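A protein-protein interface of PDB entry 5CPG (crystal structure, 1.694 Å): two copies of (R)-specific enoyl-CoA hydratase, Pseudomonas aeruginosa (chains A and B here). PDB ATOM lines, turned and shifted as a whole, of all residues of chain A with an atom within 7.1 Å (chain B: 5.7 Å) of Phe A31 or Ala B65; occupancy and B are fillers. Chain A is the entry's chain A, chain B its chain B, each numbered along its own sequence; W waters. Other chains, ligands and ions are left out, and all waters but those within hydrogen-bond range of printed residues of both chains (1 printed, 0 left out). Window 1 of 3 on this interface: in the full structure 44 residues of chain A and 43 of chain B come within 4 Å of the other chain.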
ATOM      1  N   GLU A  25       8.613  -8.317 -12.975  1.00  0.00           N
ATOM      2  CA  GLU A  25       9.281  -7.209 -12.313  1.00  0.00           C
ATOM      3  C   GLU A  25       9.368  -6.003 -13.250  1.00  0.00           C
ATOM      4  O   GLU A  25       9.230  -4.868 -12.862  1.00  0.00           O
ATOM      5  CB  GLU A  25      10.692  -7.644 -11.890  1.00  0.00           C
ATOM      6  CG  GLU A  25      11.463  -6.511 -11.228  1.00  0.00           C
ATOM      7  CD  GLU A  25      12.857  -6.876 -10.775  1.00  0.00           C
ATOM      8  OE1 GLU A  25      13.609  -7.414 -11.613  1.00  0.00           O
ATOM      9  OE2 GLU A  25      13.191  -6.581  -9.598  1.00  0.00           O
ATOM     10  N   ARG A  26       9.606  -6.284 -14.506  1.00  0.00           N
ATOM     11  CA  ARG A  26       9.843  -5.231 -15.466  1.00  0.00           C
ATOM     12  C   ARG A  26       8.579  -4.412 -15.694  1.00  0.00           C
ATOM     13  O   ARG A  26       8.653  -3.216 -15.921  1.00  0.00           O
ATOM     14  CB  ARG A  26      10.317  -5.889 -16.754  1.00  0.00           C
ATOM     15  CG  ARG A  26      11.107  -5.081 -17.655  1.00  0.00           C
ATOM     16  CD  ARG A  26      11.708  -6.010 -18.677  1.00  0.00           C
ATOM     17  NE  ARG A  26      11.596  -5.363 -19.961  1.00  0.00           N
ATOM     18  CZ  ARG A  26      12.559  -4.640 -20.513  1.00  0.00           C
ATOM     19  NH1 ARG A  26      13.728  -4.515 -19.901  1.00  0.00           N
ATOM     20  NH2 ARG A  26      12.342  -4.055 -21.676  1.00  0.00           N
ATOM     21  N   ASP A  27       7.421  -5.064 -15.575  1.00  0.00           N
ATOM     22  CA  ASP A  27       6.131  -4.345 -15.697  1.00  0.00           C
ATOM     23  C   ASP A  27       5.938  -3.371 -14.558  1.00  0.00           C
ATOM     24  O   ASP A  27       5.490  -2.238 -14.759  1.00  0.00           O
ATOM     25  CB  ASP A  27       5.008  -5.339 -15.762  1.00  0.00           C
ATOM     26  CG  ASP A  27       5.182  -6.270 -16.943  1.00  0.00           C
ATOM     27  OD1 ASP A  27       5.052  -5.787 -18.063  1.00  0.00           O
ATOM     28  OD2 ASP A  27       5.504  -7.451 -16.769  1.00  0.00           O
ATOM     29  N   LEU A  28       6.315  -3.799 -13.362  1.00  0.00           N
ATOM     30  CA  LEU A  28       6.204  -2.935 -12.174  1.00  0.00           C
ATOM     31  C   LEU A  28       7.126  -1.765 -12.359  1.00  0.00           C
ATOM     32  O   LEU A  28       6.760  -0.633 -12.082  1.00  0.00           O
ATOM     33  CB  LEU A  28       6.542  -3.725 -10.887  1.00  0.00           C
ATOM     34  CG  LEU A  28       5.401  -4.439 -10.142  1.00  0.00           C
ATOM     35  CD1 LEU A  28       4.418  -5.067 -11.119  1.00  0.00           C
ATOM     36  CD2 LEU A  28       5.961  -5.462  -9.149  1.00  0.00           C
ATOM     37  N   GLN A  29       8.349  -2.025 -12.838  1.00  0.00           N
ATOM     38  CA  GLN A  29       9.313  -0.945 -12.990  1.00  0.00           C
ATOM     39  C   GLN A  29       8.907   0.030 -14.121  1.00  0.00           C
ATOM     40  O   GLN A  29       9.008   1.226 -13.947  1.00  0.00           O
ATOM     41  CB  GLN A  29      10.692  -1.506 -13.273  1.00  0.00           C
ATOM     42  CG  GLN A  29      11.256  -2.250 -12.088  1.00  0.00           C
ATOM     43  CD  GLN A  29      12.462  -3.065 -12.463  1.00  0.00           C
ATOM     44  OE1 GLN A  29      12.563  -3.572 -13.582  1.00  0.00           O
ATOM     45  NE2 GLN A  29      13.365  -3.232 -11.516  1.00  0.00           N
ATOM     46  N   LEU A  30       8.440  -0.490 -15.253  1.00  0.00           N
ATOM     47  CA  LEU A  30       8.028   0.383 -16.332  1.00  0.00           C
ATOM     48  C   LEU A  30       6.831   1.244 -15.893  1.00  0.00           C
ATOM     49  O   LEU A  30       6.757   2.431 -16.240  1.00  0.00           O
ATOM     50  CB  LEU A  30       7.642  -0.433 -17.591  1.00  0.00           C
ATOM     51  CG  LEU A  30       8.868  -1.084 -18.206  1.00  0.00           C
ATOM     52  CD1 LEU A  30       8.393  -2.160 -19.168  1.00  0.00           C
ATOM     53  CD2 LEU A  30       9.759  -0.046 -18.950  1.00  0.00           C
ATOM     54  N   PHE A  31       5.875   0.661 -15.160  1.00  0.00           N
ATOM     55  CA  PHE A  31       4.697   1.461 -14.841  1.00  0.00           C
ATOM     56  C   PHE A  31       5.055   2.571 -13.866  1.00  0.00           C
ATOM     57  O   PHE A  31       4.532   3.693 -13.967  1.00  0.00           O
ATOM     58  CB  PHE A  31       3.562   0.604 -14.292  1.00  0.00           C
ATOM     59  CG  PHE A  31       2.263   1.338 -14.249  1.00  0.00           C
ATOM     60  CD1 PHE A  31       1.418   1.351 -15.352  1.00  0.00           C
ATOM     61  CD2 PHE A  31       1.903   2.061 -13.130  1.00  0.00           C
ATOM     62  CE1 PHE A  31       0.211   2.077 -15.310  1.00  0.00           C
ATOM     63  CE2 PHE A  31       0.717   2.747 -13.092  1.00  0.00           C
ATOM     64  CZ  PHE A  31      -0.133   2.752 -14.189  1.00  0.00           C
ATOM     65  N   ALA A  32       5.974   2.263 -12.927  1.00  0.00           N
ATOM     66  CA  ALA A  32       6.454   3.273 -11.969  1.00  0.00           C
ATOM     67  C   ALA A  32       7.127   4.401 -12.719  1.00  0.00           C
ATOM     68  O   ALA A  32       6.929   5.587 -12.421  1.00  0.00           O
ATOM     69  CB  ALA A  32       7.436   2.670 -10.963  1.00  0.00           C
ATOM     70  N   ALA A  33       7.922   4.035 -13.716  1.00  0.00           N
ATOM     71  CA  ALA A  33       8.700   5.020 -14.445  1.00  0.00           C
ATOM     72  C   ALA A  33       7.809   5.977 -15.201  1.00  0.00           C
ATOM     73  O   ALA A  33       8.086   7.172 -15.268  1.00  0.00           O
ATOM     74  CB  ALA A  33       9.679   4.349 -15.417  1.00  0.00           C
ATOM     75  N   VAL A  34       6.755   5.465 -15.797  1.00  0.00           N
ATOM     76  CA  VAL A  34       5.953   6.333 -16.638  1.00  0.00           C
ATOM     77  C   VAL A  34       4.865   7.047 -15.812  1.00  0.00           C
ATOM     78  O   VAL A  34       4.452   8.170 -16.158  1.00  0.00           O
ATOM     79  CB  VAL A  34       5.357   5.539 -17.807  1.00  0.00           C
ATOM     80  CG1 VAL A  34       4.243   4.606 -17.314  1.00  0.00           C
ATOM     81  CG2 VAL A  34       4.879   6.551 -18.886  1.00  0.00           C
ATOM     82  N   SER A  35       4.441   6.450 -14.686  1.00  0.00           N
ATOM     83  CA  SER A  35       3.442   7.130 -13.849  1.00  0.00           C
ATOM     84  C   SER A  35       4.072   8.110 -12.861  1.00  0.00           C
ATOM     85  O   SER A  35       3.451   9.110 -12.458  1.00  0.00           O
ATOM     86  CB  SER A  35       2.603   6.094 -13.078  1.00  0.00           C
ATOM     87  OG  SER A  35       3.394   5.388 -12.135  1.00  0.00           O
ATOM     88  N   GLY A  36       5.290   7.780 -12.419  1.00  0.00           N
ATOM     89  CA  GLY A  36       5.925   8.490 -11.331  1.00  0.00           C
ATOM     90  C   GLY A  36       5.619   7.920  -9.962  1.00  0.00           C
ATOM     91  O   GLY A  36       6.060   8.468  -8.951  1.00  0.00           O
ATOM     92  N   ASP A  37       4.850   6.840  -9.930  1.00  0.00           N
ATOM     93  CA  ASP A  37       4.430   6.184  -8.663  1.00  0.00           C
ATOM     94  C   ASP A  37       5.512   5.228  -8.208  1.00  0.00           C
ATOM     95  O   ASP A  37       5.531   4.028  -8.583  1.00  0.00           O
ATOM     96  CB  ASP A  37       3.102   5.445  -8.812  1.00  0.00           C
ATOM     97  CG  ASP A  37       2.578   4.864  -7.509  1.00  0.00           C
ATOM     98  OD1 ASP A  37       3.348   4.828  -6.507  1.00  0.00           O
ATOM     99  OD2 ASP A  37       1.396   4.436  -7.496  1.00  0.00           O
ATOM    100  N   LEU A  43       8.248  -1.608  -5.949  1.00  0.00           N
ATOM    101  CA  LEU A  43       9.588  -1.567  -6.491  1.00  0.00           C
ATOM    102  C   LEU A  43      10.666  -2.264  -5.675  1.00  0.00           C
ATOM    103  O   LEU A  43      11.565  -2.835  -6.246  1.00  0.00           O
ATOM    104  CB  LEU A  43      10.028  -0.109  -6.702  1.00  0.00           C
ATOM    105  CG  LEU A  43       9.280   0.607  -7.853  1.00  0.00           C
ATOM    106  CD1 LEU A  43       9.618   2.096  -7.905  1.00  0.00           C
ATOM    107  CD2 LEU A  43       9.575  -0.051  -9.201  1.00  0.00           C
ATOM    108  N   ALA A  58       1.501  -5.078  -8.060  1.00  0.00           N
ATOM    109  CA  ALA A  58       1.411  -4.185  -9.221  1.00  0.00           C
ATOM    110  C   ALA A  58       0.607  -2.961  -8.845  1.00  0.00           C
ATOM    111  O   ALA A  58      -0.209  -2.998  -7.916  1.00  0.00           O
ATOM    112  CB  ALA A  58       0.742  -4.912 -10.397  1.00  0.00           C
ATOM    113  N   HIS A  59       0.838  -1.876  -9.562  1.00  0.00           N
ATOM    114  CA  HIS A  59      -0.035  -0.709  -9.440  1.00  0.00           C
ATOM    115  C   HIS A  59      -1.423  -1.062  -9.926  1.00  0.00           C
ATOM    116  O   HIS A  59      -1.577  -1.697 -10.962  1.00  0.00           O
ATOM    117  CB  HIS A  59       0.525   0.446 -10.266  1.00  0.00           C
ATOM    118  CG  HIS A  59       1.975   0.747  -9.999  1.00  0.00           C
ATOM    119  ND1 HIS A  59       3.004  -0.010 -10.508  1.00  0.00           N
ATOM    120  CD2 HIS A  59       2.551   1.780  -9.342  1.00  0.00           C
ATOM    121  CE1 HIS A  59       4.165   0.536 -10.156  1.00  0.00           C
ATOM    122  NE2 HIS A  59       3.911   1.627  -9.450  1.00  0.00           N
ATOM    123  N   GLY A  60      -2.449  -0.630  -9.194  1.00  0.00           N
ATOM    124  CA  GLY A  60      -3.801  -0.937  -9.634  1.00  0.00           C
ATOM    125  C   GLY A  60      -4.072  -0.499 -11.048  1.00  0.00           C
ATOM    126  O   GLY A  60      -4.723  -1.214 -11.808  1.00  0.00           O
ATOM    127  N   MET A  61      -3.561   0.680 -11.411  1.00  0.00           N
ATOM    128  CA  MET A  61      -3.845   1.242 -12.718  1.00  0.00           C
ATOM    129  C   MET A  61      -3.102   0.553 -13.875  1.00  0.00           C
ATOM    130  O   MET A  61      -3.354   0.880 -15.025  1.00  0.00           O
ATOM    131  CB  MET A  61      -3.530   2.745 -12.697  1.00  0.00           C
ATOM    132  CG  MET A  61      -3.881   3.554 -13.930  1.00  0.00           C
ATOM    133  SD  MET A  61      -5.626   3.470 -14.363  1.00  0.00           S
ATOM    134  CE  MET A  61      -6.318   4.497 -13.062  1.00  0.00           C
ATOM    135  N   LEU A  62      -2.186  -0.380 -13.567  1.00  0.00           N
ATOM    136  CA  LEU A  62      -1.602  -1.218 -14.625  1.00  0.00           C
ATOM    137  C   LEU A  62      -2.751  -1.907 -15.410  1.00  0.00           C
ATOM    138  O   LEU A  62      -2.685  -2.028 -16.642  1.00  0.00           O
ATOM    139  CB  LEU A  62      -0.622  -2.246 -14.050  1.00  0.00           C
ATOM    140  CG  LEU A  62       0.004  -3.235 -15.065  1.00  0.00           C
ATOM    141  CD1 LEU A  62       0.823  -2.497 -16.107  1.00  0.00           C
ATOM    142  CD2 LEU A  62       0.850  -4.279 -14.349  1.00  0.00           C
ATOM    143  N   SER A  63      -3.827  -2.307 -14.744  1.00  0.00           N
ATOM    144  CA  SER A  63      -4.920  -2.902 -15.494  1.00  0.00           C
ATOM    145  C   SER A  63      -5.595  -1.931 -16.459  1.00  0.00           C
ATOM    146  O   SER A  63      -6.069  -2.365 -17.502  1.00  0.00           O
ATOM    147  CB  SER A  63      -5.978  -3.470 -14.556  1.00  0.00           C
ATOM    148  OG  SER A  63      -5.489  -4.632 -13.912  1.00  0.00           O
ATOM    149  N   GLY A  64      -5.650  -0.633 -16.112  1.00  0.00           N
ATOM    150  CA  GLY A  64      -6.220   0.337 -17.041  1.00  0.00           C
ATOM    151  C   GLY A  64      -5.343   0.425 -18.273  1.00  0.00           C
ATOM    152  O   GLY A  64      -5.819   0.520 -19.369  1.00  0.00           O
ATOM    153  N   ALA A  65      -4.030   0.396 -18.073  1.00  0.00           N
ATOM    154  CA  ALA A  65      -3.131   0.361 -19.194  1.00  0.00           C
ATOM    155  C   ALA A  65      -3.367  -0.845 -20.117  1.00  0.00           C
ATOM    156  O   ALA A  65      -3.415  -0.700 -21.344  1.00  0.00           O
ATOM    157  CB  ALA A  65      -1.669   0.381 -18.690  1.00  0.00           C
ATOM    158  N   LEU A  66      -3.489  -2.025 -19.535  1.00  0.00           N
ATOM    159  CA  LEU A  66      -3.697  -3.248 -20.328  1.00  0.00           C
ATOM    160  C   LEU A  66      -5.030  -3.204 -21.066  1.00  0.00           C
ATOM    161  O   LEU A  66      -5.094  -3.547 -22.227  1.00  0.00           O
ATOM    162  CB  LEU A  66      -3.631  -4.482 -19.405  1.00  0.00           C
ATOM    163  CG  LEU A  66      -2.243  -4.653 -18.776  1.00  0.00           C
ATOM    164  CD1 LEU A  66      -2.292  -5.800 -17.783  1.00  0.00           C
ATOM    165  CD2 LEU A  66      -1.206  -4.936 -19.885  1.00  0.00           C
ATOM    166  N   PHE B  31       5.222   3.931 -21.959  1.00  0.00           N
ATOM    167  CA  PHE B  31       3.824   3.522 -21.792  1.00  0.00           C
ATOM    168  C   PHE B  31       3.504   2.434 -22.819  1.00  0.00           C
ATOM    169  O   PHE B  31       2.863   1.465 -22.511  1.00  0.00           O
ATOM    170  CB  PHE B  31       2.869   4.695 -21.949  1.00  0.00           C
ATOM    171  CG  PHE B  31       1.444   4.343 -21.540  1.00  0.00           C
ATOM    172  CD1 PHE B  31       1.049   4.519 -20.241  1.00  0.00           C
ATOM    173  CD2 PHE B  31       0.550   3.783 -22.474  1.00  0.00           C
ATOM    174  CE1 PHE B  31      -0.251   4.161 -19.833  1.00  0.00           C
ATOM    175  CE2 PHE B  31      -0.707   3.413 -22.101  1.00  0.00           C
ATOM    176  CZ  PHE B  31      -1.113   3.590 -20.769  1.00  0.00           C
ATOM    177  N   VAL B  34       4.894  -0.901 -21.527  1.00  0.00           N
ATOM    178  CA  VAL B  34       4.252  -1.579 -20.403  1.00  0.00           C
ATOM    179  C   VAL B  34       2.823  -1.989 -20.795  1.00  0.00           C
ATOM    180  O   VAL B  34       2.315  -3.032 -20.323  1.00  0.00           O
ATOM    181  CB  VAL B  34       4.268  -0.713 -19.117  1.00  0.00           C
ATOM    182  CG1 VAL B  34       3.280   0.397 -19.165  1.00  0.00           C
ATOM    183  CG2 VAL B  34       3.993  -1.617 -17.893  1.00  0.00           C
ATOM    184  N   MET B  61      -4.673   6.759 -21.891  1.00  0.00           N
ATOM    185  CA  MET B  61      -4.543   6.157 -20.585  1.00  0.00           C
ATOM    186  C   MET B  61      -3.282   6.590 -19.844  1.00  0.00           C
ATOM    187  O   MET B  61      -3.155   6.341 -18.646  1.00  0.00           O
ATOM    188  CB  MET B  61      -4.619   4.631 -20.711  1.00  0.00           C
ATOM    189  CG  MET B  61      -4.704   3.857 -19.416  1.00  0.00           C
ATOM    190  SD  MET B  61      -6.038   4.390 -18.287  1.00  0.00           S
ATOM    191  CE  MET B  61      -7.482   3.929 -19.225  1.00  0.00           C
ATOM    192  N   LEU B  62      -2.372   7.299 -20.515  1.00  0.00           N
ATOM    193  CA  LEU B  62      -1.213   7.843 -19.790  1.00  0.00           C
ATOM    194  C   LEU B  62      -1.695   8.811 -18.704  1.00  0.00           C
ATOM    195  O   LEU B  62      -1.132   8.845 -17.611  1.00  0.00           O
ATOM    196  CB  LEU B  62      -0.242   8.537 -20.759  1.00  0.00           C
ATOM    197  CG  LEU B  62       0.907   9.313 -20.092  1.00  0.00           C
ATOM    198  CD1 LEU B  62       1.776   8.384 -19.234  1.00  0.00           C
ATOM    199  CD2 LEU B  62       1.752  10.096 -21.135  1.00  0.00           C
ATOM    200  N   SER B  63      -2.761   9.572 -18.987  1.00  0.00           N
ATOM    201  CA  SER B  63      -3.369  10.441 -17.949  1.00  0.00           C
ATOM    202  C   SER B  63      -3.925   9.643 -16.783  1.00  0.00           C
ATOM    203  O   SER B  63      -3.813  10.084 -15.646  1.00  0.00           O
ATOM    204  CB  SER B  63      -4.485  11.330 -18.511  1.00  0.00           C
ATOM    205  OG  SER B  63      -3.933  12.329 -19.367  1.00  0.00           O
ATOM    206  N   GLY B  64      -4.480   8.462 -17.058  1.00  0.00           N
ATOM    207  CA  GLY B  64      -4.912   7.568 -15.988  1.00  0.00           C
ATOM    208  C   GLY B  64      -3.724   7.175 -15.085  1.00  0.00           C
ATOM    209  O   GLY B  64      -3.824   7.169 -13.836  1.00  0.00           O
ATOM    210  N   ALA B  65      -2.563   6.887 -15.696  1.00  0.00           N
ATOM    211  CA  ALA B  65      -1.385   6.534 -14.908  1.00  0.00           C
ATOM    212  C   ALA B  65      -0.958   7.723 -14.038  1.00  0.00           C
ATOM    213  O   ALA B  65      -0.632   7.587 -12.870  1.00  0.00           O
ATOM    214  CB  ALA B  65      -0.229   6.103 -15.845  1.00  0.00           C
ATOM    215  N   LEU B  66      -0.937   8.927 -14.631  1.00  0.00           N
ATOM    216  CA  LEU B  66      -0.509  10.083 -13.863  1.00  0.00           C
ATOM    217  C   LEU B  66      -1.474  10.384 -12.693  1.00  0.00           C
ATOM    218  O   LEU B  66      -1.001  10.683 -11.582  1.00  0.00           O
ATOM    219  CB  LEU B  66      -0.391  11.307 -14.769  1.00  0.00           C
ATOM    220  CG  LEU B  66       0.681  11.192 -15.832  1.00  0.00           C
ATOM    221  CD1 LEU B  66       0.476  12.428 -16.757  1.00  0.00           C
ATOM    222  CD2 LEU B  66       2.099  11.127 -15.205  1.00  0.00           C
ATOM    223  N   ILE B  67      -2.791  10.296 -12.926  1.00  0.00           N
ATOM    224  CA  ILE B  67      -3.793  10.475 -11.842  1.00  0.00           C
ATOM    225  C   ILE B  67      -3.497   9.471 -10.745  1.00  0.00           C
ATOM    226  O   ILE B  67      -3.482   9.808  -9.548  1.00  0.00           O
ATOM    227  CB  ILE B  67      -5.258  10.283 -12.385  1.00  0.00           C
ATOM    228  CG1 ILE B  67      -5.623  11.486 -13.243  1.00  0.00           C
ATOM    229  CG2 ILE B  67      -6.276  10.129 -11.239  1.00  0.00           C
ATOM    230  CD1 ILE B  67      -6.902  11.256 -14.094  1.00  0.00           C
ATOM    231  N   SER B  68      -3.245   8.223 -11.143  1.00  0.00           N
ATOM    232  CA  SER B  68      -3.098   7.185 -10.129  1.00  0.00           C
ATOM    233  C   SER B  68      -1.852   7.511  -9.260  1.00  0.00           C
ATOM    234  O   SER B  68      -1.902   7.362  -8.019  1.00  0.00           O
ATOM    235  CB  SER B  68      -3.024   5.783 -10.792  1.00  0.00           C
ATOM    236  OG  SER B  68      -1.752   5.517 -11.353  1.00  0.00           O
ATOM    237  N   ALA B  69      -0.779   8.015  -9.865  1.00  0.00           N
ATOM    238  CA  ALA B  69       0.416   8.385  -9.098  1.00  0.00           C
ATOM    239  C   ALA B  69       0.158   9.588  -8.196  1.00  0.00           C
ATOM    240  O   ALA B  69       0.708   9.679  -7.091  1.00  0.00           O
ATOM    241  CB  ALA B  69       1.593   8.703 -10.016  1.00  0.00           C
ATOM    242  N   ALA B  70      -0.589  10.549  -8.694  1.00  0.00           N
ATOM    243  CA  ALA B  70      -0.927  11.718  -7.854  1.00  0.00           C
ATOM    244  C   ALA B  70      -1.670  11.293  -6.564  1.00  0.00           C
ATOM    245  O   ALA B  70      -1.367  11.778  -5.459  1.00  0.00           O
ATOM    246  CB  ALA B  70      -1.793  12.738  -8.671  1.00  0.00           C
HETATM  247  O   HOH W   1      -0.097   4.082  -9.600  1.00  0.00           O
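Of chain B, only Ala B65 comes within 4 Å of Phe A31.
Of the printed residues of chain A, Ala B65 touches Phe A31, Ser A35 and Met A61.
Printed residues of chain A within 4 Å of Gly B64: Met A61.
Of the printed residues of chain A, Val B34 touches Asp A27 (3.5 Å), Leu A30 (3.7 Å) and Leu A62 (3.7 Å).
Printed residues of chain B within 4 Å of Val A34: Leu B62 (3.6 Å) and Leu B66 (3.9 Å).
Ala A58 touches none of the printed residues of chain B.
The nearest residue of chain B that does not touch Phe A31 is Val B34 (4.02 Å).
Water W1 lies within hydrogen-bond range of OD2 of Asp A37 and OG of Ser B68.
Leu A30 touches Val B34.
Val A34 touches Leu B62 (CG2 to CD1, 3.6 Å).
Ser A35 touches Ala B65.
O of Ser A35 touches CD2 of Leu B66 (3.7 Å).
Ala B69 touches Asp A37.
Gly B64 touches Met A61 (O to CG, 3.6 Å).
Ala B65 touches Met A61 (N to CG, 3.996 Å).
Met A61 touches Ser B68 (CB to OG, 3.6 Å).
Gly A64 touches Met B61 (O to CG, 3.5 Å).
CG of Met B61 touches N of Ala A65, 3.8 Å away.
OG of Ser A35 sits at hydrogen-bond distance from O of Phe A31 (2.7 Å).
The backbone carbonyl oxygen of Ala A32 lies within hydrogen-bond range of the backbone NH of Asp A37 (3.5 Å).
The side-chain hydroxyl (OG) of Ser A35 is in hydrogen-bond range of the backbone NH (N) of Asp A37 (3.0 Å).
The backbone carbonyl oxygen (O) of Asp A37 is in hydrogen-bond range of a ring nitrogen (NE2) of His A59 (3.0 Å).
The backbone carbonyl oxygen (O) of Ala B65 sits at hydrogen-bond distance from the side-chain hydroxyl (OG) of Ser B68 (2.8 Å).
Val A34 touches Leu B62, and with the chains exchanged Leu A62 touches Val B34.
Val A34 touches Leu B66, but with the chains exchanged Leu A66 does not touch Val B34 (4.03 Å).
Met A61 touches Gly B64, and with the chains exchanged Gly A64 touches Met B61.
Met A61 touches Ala B65, and with the chains exchanged Ala A65 touches Met B61.
8 positions are printed for both chains.
Of the 16 pairs that touch across the chains among the printed residues, 8 have their exchanged pair printed and touching as well.
Printed residues of chain B that touch a printed residue of chain A: Phe B31, Val B34, Met B61, Leu B62, Gly B64, Ala B65, Leu B66, Ser B68 and Ala B69.
Hydrophobic or aromatic side chains of chain B within 4 Å of the printed part of chain A: Phe B31, Val B34, Met B61, Leu B62, Ala B65, Leu B66 and Ala B69.
Of the 23 printed residues of chain A, 10 touch a printed residue of chain B.
Printed residues of chain A that touch a printed residue of chain B: Asp A27, Leu A30, Phe A31, Val A34, Ser A35, Asp A37, Met A61, Leu A62, Gly A64 and Ala A65.
Hydrophobic or aromatic side chains of chain A that line the printed part of chain B: Leu A30, Phe A31, Val A34, Met A61, Leu A62 and Ala A65.
Among the printed residues, 16 pairs touch across the chains.
Among the printed residues, no Asp or Glu carboxylate lies within 4 Å of a Lys or Arg side-chain nitrogen of the other chain.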
